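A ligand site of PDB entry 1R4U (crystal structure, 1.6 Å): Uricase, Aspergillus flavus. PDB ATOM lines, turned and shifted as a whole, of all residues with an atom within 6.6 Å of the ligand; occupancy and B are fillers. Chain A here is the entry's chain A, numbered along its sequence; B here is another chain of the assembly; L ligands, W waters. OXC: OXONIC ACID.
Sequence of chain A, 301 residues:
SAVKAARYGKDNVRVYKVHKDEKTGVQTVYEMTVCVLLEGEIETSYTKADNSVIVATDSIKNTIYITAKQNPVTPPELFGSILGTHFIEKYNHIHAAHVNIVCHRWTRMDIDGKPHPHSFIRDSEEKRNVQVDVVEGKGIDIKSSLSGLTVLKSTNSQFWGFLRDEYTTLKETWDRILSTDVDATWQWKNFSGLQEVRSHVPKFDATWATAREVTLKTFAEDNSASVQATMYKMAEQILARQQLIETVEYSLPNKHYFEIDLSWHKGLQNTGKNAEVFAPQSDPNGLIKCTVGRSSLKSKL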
ATOM      1  N   SER A 157      -6.161 -20.862  -1.418  1.00  0.00           N
ATOM      2  CA  SER A 157      -6.489 -19.899  -2.434  1.00  0.00           C
ATOM      3  C   SER A 157      -6.328 -20.665  -3.755  1.00  0.00           C
ATOM      4  O   SER A 157      -5.344 -21.357  -3.969  1.00  0.00           O
ATOM      5  CB  SER A 157      -5.559 -18.669  -2.394  1.00  0.00           C
ATOM      6  OG  SER A 157      -5.727 -17.903  -3.582  1.00  0.00           O
ATOM      7  N   GLN A 158      -7.295 -20.525  -4.640  1.00  0.00           N
ATOM      8  CA  GLN A 158      -7.262 -21.204  -5.925  1.00  0.00           C
ATOM      9  C   GLN A 158      -7.519 -20.169  -6.998  1.00  0.00           C
ATOM     10  O   GLN A 158      -8.063 -19.092  -6.753  1.00  0.00           O
ATOM     11  CB  GLN A 158      -8.423 -22.238  -5.971  1.00  0.00           C
ATOM     12  CG  GLN A 158      -8.334 -23.190  -4.791  1.00  0.00           C
ATOM     13  CD  GLN A 158      -9.374 -24.331  -4.865  1.00  0.00           C
ATOM     14  OE1 GLN A 158     -10.084 -24.471  -5.849  1.00  0.00           O
ATOM     15  NE2 GLN A 158      -9.495 -25.066  -3.787  1.00  0.00           N
ATOM     16  N   PHE A 159      -7.162 -20.542  -8.225  1.00  0.00           N
ATOM     17  CA  PHE A 159      -7.497 -19.700  -9.365  1.00  0.00           C
ATOM     18  C   PHE A 159      -7.450 -20.514 -10.648  1.00  0.00           C
ATOM     19  O   PHE A 159      -6.376 -20.753 -11.209  1.00  0.00           O
ATOM     20  CB  PHE A 159      -6.629 -18.436  -9.430  1.00  0.00           C
ATOM     21  CG  PHE A 159      -7.146 -17.407 -10.404  1.00  0.00           C
ATOM     22  CD1 PHE A 159      -8.414 -16.853 -10.234  1.00  0.00           C
ATOM     23  CD2 PHE A 159      -6.386 -17.024 -11.505  1.00  0.00           C
ATOM     24  CE1 PHE A 159      -8.936 -15.936 -11.173  1.00  0.00           C
ATOM     25  CE2 PHE A 159      -6.886 -16.097 -12.438  1.00  0.00           C
ATOM     26  CZ  PHE A 159      -8.175 -15.561 -12.279  1.00  0.00           C
ATOM     27  N   LEU A 170      -0.777 -18.020 -18.029  1.00  0.00           N
ATOM     28  CA  LEU A 170      -0.950 -18.444 -16.633  1.00  0.00           C
ATOM     29  C   LEU A 170      -1.528 -19.864 -16.525  1.00  0.00           C
ATOM     30  O   LEU A 170      -2.558 -20.161 -17.120  1.00  0.00           O
ATOM     31  CB  LEU A 170      -1.916 -17.465 -15.957  1.00  0.00           C
ATOM     32  CG  LEU A 170      -2.084 -17.681 -14.439  1.00  0.00           C
ATOM     33  CD1 LEU A 170      -0.775 -17.449 -13.671  1.00  0.00           C
ATOM     34  CD2 LEU A 170      -3.174 -16.726 -13.932  1.00  0.00           C
ATOM     35  N   ARG A 176      -2.459 -21.759  -4.155  1.00  0.00           N
ATOM     36  CA  ARG A 176      -1.473 -20.675  -4.333  1.00  0.00           C
ATOM     37  C   ARG A 176      -1.495 -19.846  -3.052  1.00  0.00           C
ATOM     38  O   ARG A 176      -2.379 -19.962  -2.216  1.00  0.00           O
ATOM     39  CB  ARG A 176      -1.795 -19.785  -5.539  1.00  0.00           C
ATOM     40  CG  ARG A 176      -3.100 -18.996  -5.374  1.00  0.00           C
ATOM     41  CD  ARG A 176      -3.391 -18.097  -6.571  1.00  0.00           C
ATOM     42  NE  ARG A 176      -4.600 -17.285  -6.307  1.00  0.00           N
ATOM     43  CZ  ARG A 176      -5.041 -16.305  -7.084  1.00  0.00           C
ATOM     44  NH1 ARG A 176      -4.418 -16.009  -8.217  1.00  0.00           N
ATOM     45  NH2 ARG A 176      -6.136 -15.621  -6.732  1.00  0.00           N
ATOM     46  N   LEU A 178      -1.973 -16.267  -1.233  1.00  0.00           N
ATOM     47  CA  LEU A 178      -2.738 -15.056  -1.492  1.00  0.00           C
ATOM     48  C   LEU A 178      -2.304 -14.042  -0.434  1.00  0.00           C
ATOM     49  O   LEU A 178      -2.410 -14.290   0.775  1.00  0.00           O
ATOM     50  CB  LEU A 178      -4.250 -15.341  -1.367  1.00  0.00           C
ATOM     51  CG  LEU A 178      -5.154 -14.122  -1.601  1.00  0.00           C
ATOM     52  CD1 LEU A 178      -4.864 -13.540  -2.962  1.00  0.00           C
ATOM     53  CD2 LEU A 178      -6.664 -14.486  -1.468  1.00  0.00           C
ATOM     54  N   SER A 224     -10.605 -19.533  -1.187  1.00  0.00           N
ATOM     55  CA  SER A 224     -10.842 -18.525  -2.186  1.00  0.00           C
ATOM     56  C   SER A 224     -10.822 -18.990  -3.631  1.00  0.00           C
ATOM     57  O   SER A 224      -9.864 -19.580  -4.112  1.00  0.00           O
ATOM     58  CB  SER A 224      -9.835 -17.373  -1.943  1.00  0.00           C
ATOM     59  OG  SER A 224      -9.898 -16.410  -2.963  1.00  0.00           O
ATOM     60  N   ALA A 225     -11.886 -18.649  -4.362  1.00  0.00           N
ATOM     61  CA  ALA A 225     -11.957 -18.979  -5.782  1.00  0.00           C
ATOM     62  C   ALA A 225     -11.269 -17.925  -6.657  1.00  0.00           C
ATOM     63  O   ALA A 225     -10.948 -18.183  -7.790  1.00  0.00           O
ATOM     64  CB  ALA A 225     -13.448 -19.127  -6.188  1.00  0.00           C
ATOM     65  N   SER A 226     -11.092 -16.718  -6.119  1.00  0.00           N
ATOM     66  CA  SER A 226     -10.448 -15.621  -6.835  1.00  0.00           C
ATOM     67  C   SER A 226     -10.459 -14.476  -5.802  1.00  0.00           C
ATOM     68  O   SER A 226     -11.182 -14.528  -4.814  1.00  0.00           O
ATOM     69  CB  SER A 226     -11.245 -15.179  -8.070  1.00  0.00           C
ATOM     70  OG  SER A 226     -12.512 -14.645  -7.667  1.00  0.00           O
ATOM     71  N   VAL A 227      -9.718 -13.414  -6.064  1.00  0.00           N
ATOM     72  CA  VAL A 227      -9.785 -12.289  -5.147  1.00  0.00           C
ATOM     73  C   VAL A 227     -11.192 -11.692  -5.241  1.00  0.00           C
ATOM     74  O   VAL A 227     -11.763 -11.289  -4.234  1.00  0.00           O
ATOM     75  CB  VAL A 227      -8.689 -11.233  -5.533  1.00  0.00           C
ATOM     76  CG1 VAL A 227      -8.828  -9.999  -4.655  1.00  0.00           C
ATOM     77  CG2 VAL A 227      -7.313 -11.897  -5.315  1.00  0.00           C
ATOM     78  N   GLN A 228     -11.727 -11.607  -6.465  1.00  0.00           N
ATOM     79  CA  GLN A 228     -13.079 -11.079  -6.733  1.00  0.00           C
ATOM     80  C   GLN A 228     -14.105 -11.731  -5.820  1.00  0.00           C
ATOM     81  O   GLN A 228     -14.918 -11.040  -5.154  1.00  0.00           O
ATOM     82  CB  GLN A 228     -13.447 -11.361  -8.184  1.00  0.00           C
ATOM     83  CG  GLN A 228     -12.752 -10.443  -9.229  1.00  0.00           C
ATOM     84  CD  GLN A 228     -11.430 -10.981  -9.743  1.00  0.00           C
ATOM     85  OE1 GLN A 228     -10.754 -11.767  -9.071  1.00  0.00           O
ATOM     86  NE2 GLN A 228     -11.024 -10.504 -10.927  1.00  0.00           N
ATOM     87  N   ASN A 254      -3.231  -7.999  -5.528  1.00  0.00           N
ATOM     88  CA  ASN A 254      -2.913  -9.406  -5.407  1.00  0.00           C
ATOM     89  C   ASN A 254      -1.355  -9.360  -5.468  1.00  0.00           C
ATOM     90  O   ASN A 254      -0.819  -9.040  -6.507  1.00  0.00           O
ATOM     91  CB  ASN A 254      -3.523 -10.184  -6.589  1.00  0.00           C
ATOM     92  CG  ASN A 254      -3.260 -11.690  -6.491  1.00  0.00           C
ATOM     93  OD1 ASN A 254      -2.559 -12.156  -5.576  1.00  0.00           O
ATOM     94  ND2 ASN A 254      -3.772 -12.457  -7.472  1.00  0.00           N
ATOM     95  N   HIS A 256       1.930 -10.948  -5.676  1.00  0.00           N
ATOM     96  CA  HIS A 256       2.330 -12.316  -6.098  1.00  0.00           C
ATOM     97  C   HIS A 256       3.551 -12.884  -5.411  1.00  0.00           C
ATOM     98  O   HIS A 256       4.521 -12.172  -5.195  1.00  0.00           O
ATOM     99  CB  HIS A 256       2.566 -12.285  -7.607  1.00  0.00           C
ATOM    100  CG  HIS A 256       1.390 -11.766  -8.375  1.00  0.00           C
ATOM    101  ND1 HIS A 256       0.179 -12.434  -8.404  1.00  0.00           N
ATOM    102  CD2 HIS A 256       1.244 -10.652  -9.134  1.00  0.00           C
ATOM    103  CE1 HIS A 256      -0.670 -11.746  -9.164  1.00  0.00           C
ATOM    104  NE2 HIS A 256      -0.048 -10.651  -9.605  1.00  0.00           N
ATOM    105  N   GLY A 286      -1.700  -7.548  -9.160  1.00  0.00           N
ATOM    106  CA  GLY A 286      -3.102  -7.456  -9.582  1.00  0.00           C
ATOM    107  C   GLY A 286      -3.756  -6.352  -8.718  1.00  0.00           C
ATOM    108  O   GLY A 286      -3.265  -5.987  -7.643  1.00  0.00           O
ATOM    109  N   ILE A 288      -7.739  -5.342  -7.717  1.00  0.00           N
ATOM    110  CA  ILE A 288      -9.123  -5.764  -7.902  1.00  0.00           C
ATOM    111  C   ILE A 288     -10.011  -4.871  -7.027  1.00  0.00           C
ATOM    112  O   ILE A 288      -9.728  -4.663  -5.843  1.00  0.00           O
ATOM    113  CB  ILE A 288      -9.326  -7.276  -7.435  1.00  0.00           C
ATOM    114  CG1 ILE A 288      -8.330  -8.288  -8.148  1.00  0.00           C
ATOM    115  CG2 ILE A 288     -10.768  -7.708  -7.783  1.00  0.00           C
ATOM    116  CD1 ILE A 288      -6.937  -8.270  -7.675  1.00  0.00           C
ATOM    117  N   TYR B   8     -11.044  -4.209 -12.476  1.00  0.00           N
ATOM    118  CA  TYR B   8      -9.927  -4.998 -11.975  1.00  0.00           C
ATOM    119  C   TYR B   8      -8.868  -5.050 -13.089  1.00  0.00           C
ATOM    120  O   TYR B   8      -9.166  -4.852 -14.274  1.00  0.00           O
ATOM    121  CB  TYR B   8     -10.372  -6.408 -11.592  1.00  0.00           C
ATOM    122  CG  TYR B   8     -10.490  -7.333 -12.790  1.00  0.00           C
ATOM    123  CD1 TYR B   8     -11.479  -7.137 -13.756  1.00  0.00           C
ATOM    124  CD2 TYR B   8      -9.501  -8.315 -13.031  1.00  0.00           C
ATOM    125  CE1 TYR B   8     -11.473  -7.881 -14.953  1.00  0.00           C
ATOM    126  CE2 TYR B   8      -9.522  -9.113 -14.189  1.00  0.00           C
ATOM    127  CZ  TYR B   8     -10.511  -8.867 -15.156  1.00  0.00           C
ATOM    128  OH  TYR B   8     -10.502  -9.594 -16.325  1.00  0.00           O
ATOM    129  N   GLY B   9      -7.637  -5.361 -12.710  1.00  0.00           N
ATOM    130  CA  GLY B   9      -6.615  -5.404 -13.755  1.00  0.00           C
ATOM    131  C   GLY B   9      -5.229  -5.515 -13.137  1.00  0.00           C
ATOM    132  O   GLY B   9      -5.059  -6.128 -12.094  1.00  0.00           O
ATOM    133  N   LYS B  10      -4.240  -4.915 -13.793  1.00  0.00           N
ATOM    134  CA  LYS B  10      -2.845  -5.087 -13.313  1.00  0.00           C
ATOM    135  C   LYS B  10      -2.277  -3.706 -13.111  1.00  0.00           C
ATOM    136  O   LYS B  10      -2.434  -2.858 -13.982  1.00  0.00           O
ATOM    137  CB  LYS B  10      -1.991  -5.780 -14.383  1.00  0.00           C
ATOM    138  CG  LYS B  10      -0.739  -6.509 -13.831  1.00  0.00           C
ATOM    139  CD  LYS B  10      -1.124  -7.719 -12.946  1.00  0.00           C
ATOM    140  CE  LYS B  10      -0.048  -8.778 -12.811  1.00  0.00           C
ATOM    141  NZ  LYS B  10      -0.611  -9.997 -12.088  1.00  0.00           N
ATOM    142  N   ASN B  51     -15.275 -17.786 -12.841  1.00  0.00           N
ATOM    143  CA  ASN B  51     -14.073 -17.214 -13.468  1.00  0.00           C
ATOM    144  C   ASN B  51     -14.087 -17.196 -14.989  1.00  0.00           C
ATOM    145  O   ASN B  51     -13.183 -16.653 -15.627  1.00  0.00           O
ATOM    146  CB  ASN B  51     -12.813 -17.890 -12.938  1.00  0.00           C
ATOM    147  CG  ASN B  51     -12.604 -17.639 -11.461  1.00  0.00           C
ATOM    148  OD1 ASN B  51     -13.080 -16.629 -10.928  1.00  0.00           O
ATOM    149  ND2 ASN B  51     -11.798 -18.474 -10.810  1.00  0.00           N
ATOM    150  N   ILE B  54     -13.481 -13.874 -16.573  1.00  0.00           N
ATOM    151  CA  ILE B  54     -12.271 -13.121 -16.164  1.00  0.00           C
ATOM    152  C   ILE B  54     -11.073 -13.344 -17.112  1.00  0.00           C
ATOM    153  O   ILE B  54     -10.673 -14.480 -17.358  1.00  0.00           O
ATOM    154  CB  ILE B  54     -11.810 -13.562 -14.745  1.00  0.00           C
ATOM    155  CG1 ILE B  54     -12.840 -13.149 -13.682  1.00  0.00           C
ATOM    156  CG2 ILE B  54     -10.440 -12.861 -14.382  1.00  0.00           C
ATOM    157  CD1 ILE B  54     -12.581 -13.811 -12.337  1.00  0.00           C
ATOM    158  N   VAL B  55     -10.558 -12.254 -17.644  1.00  0.00           N
ATOM    159  CA  VAL B  55      -9.281 -12.238 -18.365  1.00  0.00           C
ATOM    160  C   VAL B  55      -8.326 -12.120 -17.152  1.00  0.00           C
ATOM    161  O   VAL B  55      -8.392 -11.125 -16.415  1.00  0.00           O
ATOM    162  CB  VAL B  55      -9.201 -10.978 -19.285  1.00  0.00           C
ATOM    163  CG1 VAL B  55      -7.776 -10.787 -19.873  1.00  0.00           C
ATOM    164  CG2 VAL B  55     -10.258 -11.108 -20.441  1.00  0.00           C
ATOM    165  N   ALA B  56      -7.484 -13.124 -16.899  1.00  0.00           N
ATOM    166  CA  ALA B  56      -6.636 -13.127 -15.700  1.00  0.00           C
ATOM    167  C   ALA B  56      -5.744 -11.876 -15.693  1.00  0.00           C
ATOM    168  O   ALA B  56      -5.326 -11.426 -16.754  1.00  0.00           O
ATOM    169  CB  ALA B  56      -5.756 -14.427 -15.666  1.00  0.00           C
ATOM    170  N   THR B  57      -5.409 -11.358 -14.506  1.00  0.00           N
ATOM    171  CA  THR B  57      -4.600 -10.138 -14.499  1.00  0.00           C
ATOM    172  C   THR B  57      -3.229 -10.448 -15.101  1.00  0.00           C
ATOM    173  O   THR B  57      -2.639  -9.579 -15.746  1.00  0.00           O
ATOM    174  CB  THR B  57      -4.450  -9.494 -13.113  1.00  0.00           C
ATOM    175  OG1 THR B  57      -3.717 -10.360 -12.238  1.00  0.00           O
ATOM    176  CG2 THR B  57      -5.895  -9.208 -12.503  1.00  0.00           C
ATOM    177  N   ASP B  58      -2.784 -11.702 -14.971  1.00  0.00           N
ATOM    178  CA  ASP B  58      -1.494 -12.067 -15.591  1.00  0.00           C
ATOM    179  C   ASP B  58      -1.576 -11.869 -17.095  1.00  0.00           C
ATOM    180  O   ASP B  58      -0.618 -11.451 -17.741  1.00  0.00           O
ATOM    181  CB  ASP B  58      -1.167 -13.532 -15.302  1.00  0.00           C
ATOM    182  CG  ASP B  58       0.249 -13.902 -15.745  1.00  0.00           C
ATOM    183  OD1 ASP B  58       1.208 -13.432 -15.073  1.00  0.00           O
ATOM    184  OD2 ASP B  58       0.404 -14.593 -16.792  1.00  0.00           O
ATOM    185  N   SER B  59      -2.748 -12.196 -17.680  1.00  0.00           N
ATOM    186  CA  SER B  59      -2.896 -12.012 -19.136  1.00  0.00           C
ATOM    187  C   SER B  59      -2.923 -10.556 -19.552  1.00  0.00           C
ATOM    188  O   SER B  59      -2.497 -10.199 -20.653  1.00  0.00           O
ATOM    189  CB  SER B  59      -4.184 -12.741 -19.639  1.00  0.00           C
ATOM    190  OG  SER B  59      -4.103 -14.103 -19.230  1.00  0.00           O
ATOM    191  N   ILE B  60      -3.426  -9.699 -18.670  1.00  0.00           N
ATOM    192  CA  ILE B  60      -3.437  -8.268 -18.946  1.00  0.00           C
ATOM    193  C   ILE B  60      -1.974  -7.818 -18.998  1.00  0.00           C
ATOM    194  O   ILE B  60      -1.606  -7.024 -19.838  1.00  0.00           O
ATOM    195  CB  ILE B  60      -4.248  -7.497 -17.860  1.00  0.00           C
ATOM    196  CG1 ILE B  60      -5.737  -7.902 -17.994  1.00  0.00           C
ATOM    197  CG2 ILE B  60      -4.123  -5.965 -18.037  1.00  0.00           C
ATOM    198  CD1 ILE B  60      -6.625  -7.460 -16.802  1.00  0.00           C
HETATM  199  N1  OXC L   1      -8.074 -12.616 -10.099  1.00  0.00           N
HETATM  200  C2  OXC L   1      -7.285 -13.356  -9.274  1.00  0.00           C
HETATM  201  O2  OXC L   1      -7.695 -13.729  -8.165  1.00  0.00           O
HETATM  202  N3  OXC L   1      -6.035 -13.728  -9.715  1.00  0.00           N
HETATM  203  C4  OXC L   1      -5.637 -13.309 -10.907  1.00  0.00           C
HETATM  204  N5  OXC L   1      -6.384 -12.541 -11.714  1.00  0.00           N
HETATM  205  C6  OXC L   1      -7.725 -12.153 -11.339  1.00  0.00           C
HETATM  206  O6  OXC L   1      -8.484 -11.462 -11.991  1.00  0.00           O
HETATM  207  CG  OXC L   1      -4.242 -13.638 -11.359  1.00  0.00           C
HETATM  208  OD1 OXC L   1      -3.859 -13.037 -12.392  1.00  0.00           O
HETATM  209  OD2 OXC L   1      -3.539 -14.409 -10.689  1.00  0.00           O
HETATM  210  O   HOH W   1      -1.412 -15.488 -10.342  1.00  0.00           O
HETATM  211  O   HOH W   2      -4.548 -10.476  -9.473  1.00  0.00           O
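Water W2 bridges the side-chain hydroxyl of Thr 57 of chain B (2.9 Å) and the side-chain amide nitrogen of Asn 254 (2.9 Å).
CE2 of Phe 159 touches C4 of the ligand, 3.4 Å away. CA of Ser 226 touches O2 of the ligand, at 3.6 Å. CE2 of Tyr 8 of chain B touches O6 of the ligand, 3.4 Å away. CG2 of Ile 54 of chain B touches O6 of the ligand, at 3.4 Å. Ala 56 of chain B touches the ligand (C to OD1, 3.97 Å). Hydrophobic or aromatic side chains within 4 Å of the ligand: Phe 159, Val 227, Tyr 8 of chain B and Ile 54 of chain B. 11 residues have an atom within 4 Å of the ligand: Phe 159, Arg 176, Ser 226, Val 227, Gln 228, Asn 254, Tyr 8 of chain B, Ile 54 of chain B, Ala 56 of chain B, Thr 57 of chain B and Asp 58 of chain B. The nearest printed residue that does not touch the ligand is Leu 170 (4.002 Å).
The side-chain hydroxyl (OG) of Ser 224 sits at hydrogen-bond distance from the backbone carbonyl oxygen (O) of Ser 226, 2.9 Å away. N of Asn 254 lies within hydrogen-bond range of O of Gly 286 (2.9 Å). OH of Tyr 8 of chain B sits at hydrogen-bond distance from O of Val 55 of chain B, at 2.6 Å. N of Gln 228 lies close to OG of Ser 226 (3.4 Å). N of Arg 176 sits at hydrogen-bond distance from O of Ser 157 (2.9 Å). The side-chain hydroxyl (OG1) of Thr 57 of chain B is in hydrogen-bond range of the side-chain amino group (NZ) of Lys 10 of chain B (3.1 Å).
The backbone NH (N) of Thr 57 of chain B lies within hydrogen-bond range of an oxygen (OD1) of the ligand. An oxygen (OD2) of the ligand lies within salt-bridge range of the guanidinium group (NH1) of Arg 176, at 3.1 Å. An oxygen (OD1) of the ligand lies within hydrogen-bond range of the backbone NH of Asp 58 of chain B (3.1 Å). OG1 of Thr 57 of chain B sits at hydrogen-bond distance from OD1 of the ligand. An oxygen (O2) of the ligand is in hydrogen-bond range of the backbone NH of Val 227 (2.9 Å). The side-chain amide nitrogen of Gln 228 is in hydrogen-bond range of an oxygen (O6) of the ligand (2.9 Å). A nitrogen (N3) of the ligand sits close to the side-chain amide nitrogen (ND2) of Asn 254, at 3.4 Å.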
